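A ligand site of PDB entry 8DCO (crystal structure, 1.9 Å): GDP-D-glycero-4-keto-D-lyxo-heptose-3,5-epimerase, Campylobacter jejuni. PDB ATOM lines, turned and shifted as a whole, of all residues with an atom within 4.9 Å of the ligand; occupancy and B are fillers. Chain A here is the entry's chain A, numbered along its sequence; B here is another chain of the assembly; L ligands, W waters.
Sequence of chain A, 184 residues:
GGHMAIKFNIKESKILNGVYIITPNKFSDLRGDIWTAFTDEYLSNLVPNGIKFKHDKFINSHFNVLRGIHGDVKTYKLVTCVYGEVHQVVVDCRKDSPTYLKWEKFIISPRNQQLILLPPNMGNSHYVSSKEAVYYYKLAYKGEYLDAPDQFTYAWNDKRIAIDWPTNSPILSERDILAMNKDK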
ATOM      1  N   LYS A  57      -3.051 -27.069 -23.963  1.00  0.00           N
ATOM      2  CA  LYS A  57      -3.876 -27.625 -22.862  1.00  0.00           C
ATOM      3  C   LYS A  57      -5.263 -28.015 -23.374  1.00  0.00           C
ATOM      4  O   LYS A  57      -5.811 -27.383 -24.293  1.00  0.00           O
ATOM      5  CB  LYS A  57      -4.056 -26.590 -21.744  1.00  0.00           C
ATOM      6  CG  LYS A  57      -2.776 -26.059 -21.130  1.00  0.00           C
ATOM      7  CD  LYS A  57      -3.004 -25.287 -19.858  1.00  0.00           C
ATOM      8  CE  LYS A  57      -3.358 -26.164 -18.680  1.00  0.00           C
ATOM      9  NZ  LYS A  57      -3.750 -25.355 -17.485  1.00  0.00           N
ATOM     10  N   ILE A  59      -9.208 -28.991 -21.620  1.00  0.00           N
ATOM     11  CA  ILE A  59     -10.107 -28.906 -20.436  1.00  0.00           C
ATOM     12  C   ILE A  59     -11.425 -29.550 -20.864  1.00  0.00           C
ATOM     13  O   ILE A  59     -12.114 -28.967 -21.735  1.00  0.00           O
ATOM     14  CB  ILE A  59     -10.291 -27.449 -19.932  1.00  0.00           C
ATOM     15  CG1 ILE A  59      -8.975 -26.687 -19.825  1.00  0.00           C
ATOM     16  CG2 ILE A  59     -11.060 -27.449 -18.627  1.00  0.00           C
ATOM     17  CD1 ILE A  59      -9.045 -25.372 -19.020  1.00  0.00           C
ATOM     18  N   ARG A  67     -16.018 -21.994 -15.472  1.00  0.00           N
ATOM     19  CA  ARG A  67     -14.637 -21.743 -14.970  1.00  0.00           C
ATOM     20  C   ARG A  67     -14.298 -20.283 -15.268  1.00  0.00           C
ATOM     21  O   ARG A  67     -14.441 -19.894 -16.428  1.00  0.00           O
ATOM     22  CB  ARG A  67     -13.642 -22.688 -15.652  1.00  0.00           C
ATOM     23  CG  ARG A  67     -14.013 -24.169 -15.580  1.00  0.00           C
ATOM     24  CD  ARG A  67     -13.027 -25.025 -16.367  1.00  0.00           C
ATOM     25  NE  ARG A  67     -13.361 -26.439 -16.313  1.00  0.00           N
ATOM     26  CZ  ARG A  67     -12.720 -27.356 -15.576  1.00  0.00           C
ATOM     27  NH1 ARG A  67     -11.683 -27.023 -14.824  1.00  0.00           N
ATOM     28  NH2 ARG A  67     -13.128 -28.612 -15.587  1.00  0.00           N
ATOM     29  N   HIS A  70     -10.464 -15.869 -14.837  1.00  0.00           N
ATOM     30  CA  HIS A  70      -9.030 -16.012 -14.492  1.00  0.00           C
ATOM     31  C   HIS A  70      -8.154 -15.217 -15.460  1.00  0.00           C
ATOM     32  O   HIS A  70      -8.513 -15.085 -16.629  1.00  0.00           O
ATOM     33  CB  HIS A  70      -8.627 -17.482 -14.406  1.00  0.00           C
ATOM     34  CG  HIS A  70      -9.511 -18.311 -13.539  1.00  0.00           C
ATOM     35  ND1 HIS A  70      -9.587 -19.687 -13.666  1.00  0.00           N
ATOM     36  CD2 HIS A  70     -10.354 -17.982 -12.532  1.00  0.00           C
ATOM     37  CE1 HIS A  70     -10.459 -20.166 -12.778  1.00  0.00           C
ATOM     38  NE2 HIS A  70     -10.959 -19.127 -12.099  1.00  0.00           N
ATOM     39  N   TYR A 145       5.232 -21.119 -16.230  1.00  0.00           N
ATOM     40  CA  TYR A 145       3.761 -21.139 -16.233  1.00  0.00           C
ATOM     41  C   TYR A 145       3.285 -20.551 -14.905  1.00  0.00           C
ATOM     42  O   TYR A 145       3.772 -20.969 -13.831  1.00  0.00           O
ATOM     43  CB  TYR A 145       3.242 -22.557 -16.481  1.00  0.00           C
ATOM     44  CG  TYR A 145       1.742 -22.657 -16.423  1.00  0.00           C
ATOM     45  CD1 TYR A 145       0.943 -22.097 -17.409  1.00  0.00           C
ATOM     46  CD2 TYR A 145       1.112 -23.256 -15.341  1.00  0.00           C
ATOM     47  CE1 TYR A 145      -0.441 -22.154 -17.323  1.00  0.00           C
ATOM     48  CE2 TYR A 145      -0.267 -23.325 -15.236  1.00  0.00           C
ATOM     49  CZ  TYR A 145      -1.050 -22.775 -16.236  1.00  0.00           C
ATOM     50  OH  TYR A 145      -2.397 -22.860 -16.133  1.00  0.00           O
ATOM     51  N   ASP A 147       0.593 -20.727 -12.458  1.00  0.00           N
ATOM     52  CA  ASP A 147      -0.543 -21.539 -11.950  1.00  0.00           C
ATOM     53  C   ASP A 147      -1.431 -20.599 -11.110  1.00  0.00           C
ATOM     54  O   ASP A 147      -1.029 -19.422 -10.918  1.00  0.00           O
ATOM     55  CB  ASP A 147      -0.023 -22.771 -11.193  1.00  0.00           C
ATOM     56  CG  ASP A 147      -0.907 -23.996 -11.259  1.00  0.00           C
ATOM     57  OD1 ASP A 147      -1.975 -23.958 -11.925  1.00  0.00           O
ATOM     58  OD2 ASP A 147      -0.498 -25.004 -10.684  1.00  0.00           O
ATOM     59  N   ALA A 148      -2.587 -21.100 -10.644  1.00  0.00           N
ATOM     60  CA  ALA A 148      -3.562 -20.412  -9.757  1.00  0.00           C
ATOM     61  C   ALA A 148      -2.924 -19.373  -8.829  1.00  0.00           C
ATOM     62  O   ALA A 148      -3.332 -18.216  -8.858  1.00  0.00           O
ATOM     63  CB  ALA A 148      -4.346 -21.457  -8.971  1.00  0.00           C
ATOM     64  N   GLN A 151      -2.178 -16.050 -10.558  1.00  0.00           N
ATOM     65  CA  GLN A 151      -3.277 -15.537 -11.395  1.00  0.00           C
ATOM     66  C   GLN A 151      -4.166 -14.691 -10.484  1.00  0.00           C
ATOM     67  O   GLN A 151      -4.133 -14.922  -9.248  1.00  0.00           O
ATOM     68  CB  GLN A 151      -4.090 -16.679 -12.009  1.00  0.00           C
ATOM     69  CG  GLN A 151      -3.280 -17.648 -12.868  1.00  0.00           C
ATOM     70  CD  GLN A 151      -4.063 -18.866 -13.312  1.00  0.00           C
ATOM     71  OE1 GLN A 151      -5.289 -18.887 -13.289  1.00  0.00           O
ATOM     72  NE2 GLN A 151      -3.354 -19.895 -13.727  1.00  0.00           N
ATOM     73  N   SER A 173     -15.779 -24.227  -8.951  1.00  0.00           N
ATOM     74  CA  SER A 173     -14.654 -24.673  -8.097  1.00  0.00           C
ATOM     75  C   SER A 173     -14.619 -23.808  -6.827  1.00  0.00           C
ATOM     76  O   SER A 173     -15.288 -22.769  -6.795  1.00  0.00           O
ATOM     77  CB  SER A 173     -13.344 -24.557  -8.833  1.00  0.00           C
ATOM     78  OG  SER A 173     -12.918 -23.204  -8.913  1.00  0.00           O
ATOM     79  N   ARG A 175     -12.060 -21.959  -5.743  1.00  0.00           N
ATOM     80  CA  ARG A 175     -11.462 -20.659  -6.158  1.00  0.00           C
ATOM     81  C   ARG A 175     -12.572 -19.724  -6.679  1.00  0.00           C
ATOM     82  O   ARG A 175     -12.601 -18.536  -6.289  1.00  0.00           O
ATOM     83  CB  ARG A 175     -10.287 -20.861  -7.122  1.00  0.00           C
ATOM     84  CG  ARG A 175     -10.217 -19.846  -8.270  1.00  0.00           C
ATOM     85  CD  ARG A 175      -8.899 -19.174  -8.591  1.00  0.00           C
ATOM     86  NE  ARG A 175      -8.216 -19.856  -9.680  1.00  0.00           N
ATOM     87  CZ  ARG A 175      -7.479 -19.290 -10.638  1.00  0.00           C
ATOM     88  NH1 ARG A 175      -7.310 -17.969 -10.734  1.00  0.00           N
ATOM     89  NH2 ARG A 175      -6.919 -20.080 -11.540  1.00  0.00           N
ATOM     90  N   ASP A 176     -13.515 -20.218  -7.488  1.00  0.00           N
ATOM     91  CA  ASP A 176     -14.459 -19.322  -8.197  1.00  0.00           C
ATOM     92  C   ASP A 176     -15.621 -18.942  -7.244  1.00  0.00           C
ATOM     93  O   ASP A 176     -16.131 -17.822  -7.382  1.00  0.00           O
ATOM     94  CB  ASP A 176     -14.878 -19.944  -9.521  1.00  0.00           C
ATOM     95  CG  ASP A 176     -13.696 -20.044 -10.474  1.00  0.00           C
ATOM     96  OD1 ASP A 176     -12.692 -19.343 -10.182  1.00  0.00           O
ATOM     97  OD2 ASP A 176     -13.774 -20.827 -11.485  1.00  0.00           O
ATOM     98  N   MET B   4      -0.716 -29.666  -7.893  1.00  0.00           N
ATOM     99  CA  MET B   4      -0.314 -30.688  -8.919  1.00  0.00           C
ATOM    100  C   MET B   4       0.461 -30.008 -10.063  1.00  0.00           C
ATOM    101  O   MET B   4      -0.172 -29.260 -10.852  1.00  0.00           O
ATOM    102  CB  MET B   4      -1.543 -31.402  -9.493  1.00  0.00           C
ATOM    103  CG  MET B   4      -1.196 -32.618 -10.344  1.00  0.00           C
ATOM    104  SD  MET B   4      -2.647 -33.524 -10.972  1.00  0.00           S
ATOM    105  CE  MET B   4      -1.966 -35.174 -11.061  1.00  0.00           C
ATOM    106  N   ALA B   5       1.783 -30.264 -10.148  1.00  0.00           N
ATOM    107  CA  ALA B   5       2.681 -29.828 -11.245  1.00  0.00           C
ATOM    108  C   ALA B   5       2.374 -30.627 -12.518  1.00  0.00           C
ATOM    109  O   ALA B   5       2.074 -31.838 -12.412  1.00  0.00           O
ATOM    110  CB  ALA B   5       4.128 -29.995 -10.838  1.00  0.00           C
ATOM    111  N   ILE B   6       2.433 -29.971 -13.692  1.00  0.00           N
ATOM    112  CA  ILE B   6       2.402 -30.592 -15.042  1.00  0.00           C
ATOM    113  C   ILE B   6       3.515 -31.648 -15.147  1.00  0.00           C
ATOM    114  O   ILE B   6       4.696 -31.313 -14.940  1.00  0.00           O
ATOM    115  CB  ILE B   6       2.557 -29.513 -16.131  1.00  0.00           C
ATOM    116  CG1 ILE B   6       1.398 -28.521 -16.111  1.00  0.00           C
ATOM    117  CG2 ILE B   6       2.726 -30.152 -17.518  1.00  0.00           C
ATOM    118  CD1 ILE B   6       1.673 -27.224 -16.858  1.00  0.00           C
ATOM    119  N   ASN B  25      -0.083 -36.223 -16.825  1.00  0.00           N
ATOM    120  CA  ASN B  25      -1.003 -36.244 -15.671  1.00  0.00           C
ATOM    121  C   ASN B  25      -2.221 -35.370 -16.017  1.00  0.00           C
ATOM    122  O   ASN B  25      -2.194 -34.700 -17.091  1.00  0.00           O
ATOM    123  CB  ASN B  25      -0.335 -35.892 -14.330  1.00  0.00           C
ATOM    124  CG  ASN B  25       0.307 -34.529 -14.297  1.00  0.00           C
ATOM    125  OD1 ASN B  25       0.310 -33.814 -15.297  1.00  0.00           O
ATOM    126  ND2 ASN B  25       0.882 -34.175 -13.161  1.00  0.00           N
ATOM    127  N   LYS B  26      -3.244 -35.429 -15.161  1.00  0.00           N
ATOM    128  CA  LYS B  26      -4.548 -34.721 -15.272  1.00  0.00           C
ATOM    129  C   LYS B  26      -4.962 -34.275 -13.871  1.00  0.00           C
ATOM    130  O   LYS B  26      -4.742 -35.038 -12.909  1.00  0.00           O
ATOM    131  CB  LYS B  26      -5.632 -35.642 -15.831  1.00  0.00           C
ATOM    132  CG  LYS B  26      -5.353 -36.233 -17.201  1.00  0.00           C
ATOM    133  CD  LYS B  26      -6.623 -36.579 -18.010  1.00  0.00           C
ATOM    134  CE  LYS B  26      -6.324 -36.824 -19.484  1.00  0.00           C
ATOM    135  NZ  LYS B  26      -7.536 -37.111 -20.310  1.00  0.00           N
ATOM    136  N   PHE B  27      -5.514 -33.074 -13.751  1.00  0.00           N
ATOM    137  CA  PHE B  27      -6.265 -32.625 -12.543  1.00  0.00           C
ATOM    138  C   PHE B  27      -7.741 -32.884 -12.816  1.00  0.00           C
ATOM    139  O   PHE B  27      -8.264 -32.383 -13.843  1.00  0.00           O
ATOM    140  CB  PHE B  27      -5.985 -31.169 -12.207  1.00  0.00           C
ATOM    141  CG  PHE B  27      -6.697 -30.713 -10.958  1.00  0.00           C
ATOM    142  CD1 PHE B  27      -6.076 -30.783  -9.725  1.00  0.00           C
ATOM    143  CD2 PHE B  27      -8.003 -30.227 -11.023  1.00  0.00           C
ATOM    144  CE1 PHE B  27      -6.736 -30.378  -8.569  1.00  0.00           C
ATOM    145  CE2 PHE B  27      -8.662 -29.831  -9.872  1.00  0.00           C
ATOM    146  CZ  PHE B  27      -8.027 -29.903  -8.649  1.00  0.00           C
ATOM    147  N   ARG B  31     -15.893 -30.721 -11.965  1.00  0.00           N
ATOM    148  CA  ARG B  31     -16.154 -29.983 -13.222  1.00  0.00           C
ATOM    149  C   ARG B  31     -15.692 -30.822 -14.404  1.00  0.00           C
ATOM    150  O   ARG B  31     -16.235 -30.635 -15.492  1.00  0.00           O
ATOM    151  CB  ARG B  31     -15.441 -28.623 -13.181  1.00  0.00           C
ATOM    152  CG  ARG B  31     -15.895 -27.731 -12.023  1.00  0.00           C
ATOM    153  CD  ARG B  31     -15.042 -26.483 -11.927  1.00  0.00           C
ATOM    154  NE  ARG B  31     -13.650 -26.829 -11.674  1.00  0.00           N
ATOM    155  CZ  ARG B  31     -12.597 -26.030 -11.828  1.00  0.00           C
ATOM    156  NH1 ARG B  31     -12.745 -24.782 -12.239  1.00  0.00           N
ATOM    157  NH2 ARG B  31     -11.396 -26.494 -11.567  1.00  0.00           N
ATOM    158  N   ILE B  34      -8.464 -31.223 -16.400  1.00  0.00           N
ATOM    159  CA  ILE B  34      -7.489 -30.296 -17.030  1.00  0.00           C
ATOM    160  C   ILE B  34      -6.212 -31.080 -17.321  1.00  0.00           C
ATOM    161  O   ILE B  34      -5.719 -31.792 -16.426  1.00  0.00           O
ATOM    162  CB  ILE B  34      -7.167 -29.087 -16.135  1.00  0.00           C
ATOM    163  CG1 ILE B  34      -8.424 -28.427 -15.546  1.00  0.00           C
ATOM    164  CG2 ILE B  34      -6.306 -28.086 -16.902  1.00  0.00           C
ATOM    165  CD1 ILE B  34      -8.141 -27.564 -14.325  1.00  0.00           C
ATOM    166  N   TRP B  35      -5.667 -30.953 -18.521  1.00  0.00           N
ATOM    167  CA  TRP B  35      -4.311 -31.487 -18.801  1.00  0.00           C
ATOM    168  C   TRP B  35      -3.586 -30.708 -19.891  1.00  0.00           C
ATOM    169  O   TRP B  35      -4.246 -29.996 -20.727  1.00  0.00           O
ATOM    170  CB  TRP B  35      -4.389 -32.987 -19.115  1.00  0.00           C
ATOM    171  CG  TRP B  35      -5.250 -33.359 -20.279  1.00  0.00           C
ATOM    172  CD1 TRP B  35      -6.625 -33.398 -20.316  1.00  0.00           C
ATOM    173  CD2 TRP B  35      -4.802 -33.747 -21.591  1.00  0.00           C
ATOM    174  NE1 TRP B  35      -7.044 -33.829 -21.544  1.00  0.00           N
ATOM    175  CE2 TRP B  35      -5.952 -34.039 -22.351  1.00  0.00           C
ATOM    176  CE3 TRP B  35      -3.545 -33.897 -22.190  1.00  0.00           C
ATOM    177  CZ2 TRP B  35      -5.879 -34.465 -23.670  1.00  0.00           C
ATOM    178  CZ3 TRP B  35      -3.471 -34.339 -23.483  1.00  0.00           C
ATOM    179  CH2 TRP B  35      -4.626 -34.607 -24.227  1.00  0.00           C
ATOM    180  N   THR B  36      -2.265 -30.858 -19.878  1.00  0.00           N
ATOM    181  CA  THR B  36      -1.293 -30.243 -20.815  1.00  0.00           C
ATOM    182  C   THR B  36      -0.821 -31.325 -21.797  1.00  0.00           C
ATOM    183  O   THR B  36      -0.290 -32.355 -21.338  1.00  0.00           O
ATOM    184  CB  THR B  36      -0.127 -29.604 -20.048  1.00  0.00           C
ATOM    185  OG1 THR B  36      -0.618 -28.516 -19.270  1.00  0.00           O
ATOM    186  CG2 THR B  36       0.967 -29.151 -20.972  1.00  0.00           C
HETATM  187  P1  LIG L   1      -9.634 -23.566 -13.890  1.00  0.00           P
HETATM  188  O1  LIG L   1     -10.507 -23.336 -12.660  1.00  0.00           O
HETATM  189  O2  LIG L   1     -10.084 -24.687 -14.815  1.00  0.00           O
HETATM  190  O3  LIG L   1      -9.323 -22.288 -14.652  1.00  0.00           O
HETATM  191  O4  LIG L   1      -8.255 -24.185 -13.266  1.00  0.00           O
HETATM  192  P2  LIG L   1      -7.146 -23.496 -12.293  1.00  0.00           P
HETATM  193  O5  LIG L   1      -7.840 -22.777 -11.169  1.00  0.00           O
HETATM  194  O6  LIG L   1      -6.118 -22.766 -13.145  1.00  0.00           O
HETATM  195  O7  LIG L   1      -6.389 -24.756 -11.582  1.00  0.00           O
HETATM  196  C1  LIG L   1      -7.102 -25.854 -11.012  1.00  0.00           C
HETATM  197  C2  LIG L   1      -6.174 -26.990 -10.576  1.00  0.00           C
HETATM  198  O8  LIG L   1      -5.616 -27.759 -11.665  1.00  0.00           O
HETATM  199  C3  LIG L   1      -4.939 -26.544  -9.822  1.00  0.00           C
HETATM  200  O9  LIG L   1      -4.665 -27.549  -8.860  1.00  0.00           O
HETATM  201  C4  LIG L   1      -3.779 -26.613 -10.773  1.00  0.00           C
HETATM  202  O10 LIG L   1      -2.572 -26.750 -10.017  1.00  0.00           O
HETATM  203  C5  LIG L   1      -4.185 -27.819 -11.604  1.00  0.00           C
HETATM  204  N1  LIG L   1      -3.745 -27.789 -13.030  1.00  0.00           N
HETATM  205  C6  LIG L   1      -3.914 -26.736 -13.862  1.00  0.00           C
HETATM  206  N2  LIG L   1      -3.416 -26.990 -15.103  1.00  0.00           N
HETATM  207  C7  LIG L   1      -2.935 -28.229 -15.070  1.00  0.00           C
HETATM  208  C8  LIG L   1      -2.289 -29.094 -16.073  1.00  0.00           C
HETATM  209  O11 LIG L   1      -2.086 -28.687 -17.261  1.00  0.00           O
HETATM  210  N3  LIG L   1      -1.967 -30.328 -15.646  1.00  0.00           N
HETATM  211  C9  LIG L   1      -2.157 -30.755 -14.366  1.00  0.00           C
HETATM  212  N4  LIG L   1      -1.760 -32.005 -14.040  1.00  0.00           N
HETATM  213  N5  LIG L   1      -2.756 -30.009 -13.406  1.00  0.00           N
HETATM  214  C10 LIG L   1      -3.139 -28.755 -13.713  1.00  0.00           C
HETATM  215  O   HOH W   1      -1.339 -32.298 -17.512  1.00  0.00           O
HETATM  216  O   HOH W   2     -10.478 -23.240  -9.925  1.00  0.00           O
HETATM  217  O   HOH W   3     -10.287 -22.039 -17.104  1.00  0.00           O
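A ring nitrogen (ND1) of His 70 is in hydrogen-bond range of the guanidinium group (NH2) of Arg 175 (3.4 Å). A ring nitrogen (NE2) of His 70 is in hydrogen-bond range of the side-chain carboxylate of Asp 176 (2.6 Å). NH2 of Arg 175 sits at hydrogen-bond distance from OE1 of Gln 151, 2.7 Å away. NZ of Lys 57 lies within hydrogen-bond range of OH of Tyr 145 (3.1 Å). The backbone carbonyl oxygen (O) of Ala 5 of chain B lies within hydrogen-bond range of the side-chain amide nitrogen (ND2) of Asn 25 of chain B (2.7 Å). The backbone carbonyl oxygen (O) of Phe 27 of chain B sits at hydrogen-bond distance from the backbone NH (N) of Ile 34 of chain B (2.8 Å). The side-chain amide nitrogen of Gln 151 lies close to the backbone NH of Ala 148 (3.4 Å).
Residues that only touch the ligand: Gln 151 (3.97 Å), Ile 6 of chain B (3.7 Å), Lys 26 of chain B (3.9 Å), Phe 27 of chain B (3.2 Å), Ile 34 of chain B (3.5 Å) and Trp 35 of chain B (3.6 Å). Hydrophobic or aromatic side chains that line the ligand: His 70, Met 4 of chain B, Ile 6 of chain B, Phe 27 of chain B and Ile 34 of chain B. Within 4 Å of the ligand: Lys 57, Arg 67, His 70, Asp 147, Gln 151, Arg 175, Met 4 of chain B, Ile 6 of chain B, Asn 25 of chain B, Lys 26 of chain B, Phe 27 of chain B, Arg 31 of chain B, Ile 34 of chain B, Trp 35 of chain B and Thr 36 of chain B. The nearest printed residue that does not touch the ligand is Ala 5 of chain B (4.2 Å).
Water W2 bridges OG of Ser 173 (2.6 Å) and O1 of the ligand (2.7 Å). Water W1 lies within hydrogen-bond range of O of Asn 25 of chain B (2.6 Å), N3 of the ligand (2.8 Å) and N of Thr 36 of chain B (2.9 Å).
O11 of the ligand is in hydrogen-bond range of N of Thr 36 of chain B, 3.4 Å away. OG1 of Thr 36 of chain B sits at hydrogen-bond distance from O11 of the ligand. The guanidinium group of Arg 31 of chain B lies within salt-bridge range of an oxygen (O1) of the ligand. OD2 of Asp 147 lies within hydrogen-bond range of O10 of the ligand (2.8 Å). A ring nitrogen (ND1) of His 70 lies within hydrogen-bond range of an oxygen (O3) of the ligand, at 2.8 Å. An oxygen (O2) of the ligand is in salt-bridge range of the guanidinium group (NH1) of Arg 67, 2.8 Å away. NH2 of Arg 175 lies within salt-bridge range of O5 of the ligand (2.9 Å). The side-chain amino group (NZ) of Lys 57 lies within hydrogen-bond range of a nitrogen (N2) of the ligand (2.9 Å). N4 of the ligand lies within hydrogen-bond range of OD1 of Asn 25 of chain B, at 3.0 Å. SD of Met 4 of chain B sits at hydrogen-bond distance from N4 of the ligand (3.5 Å).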
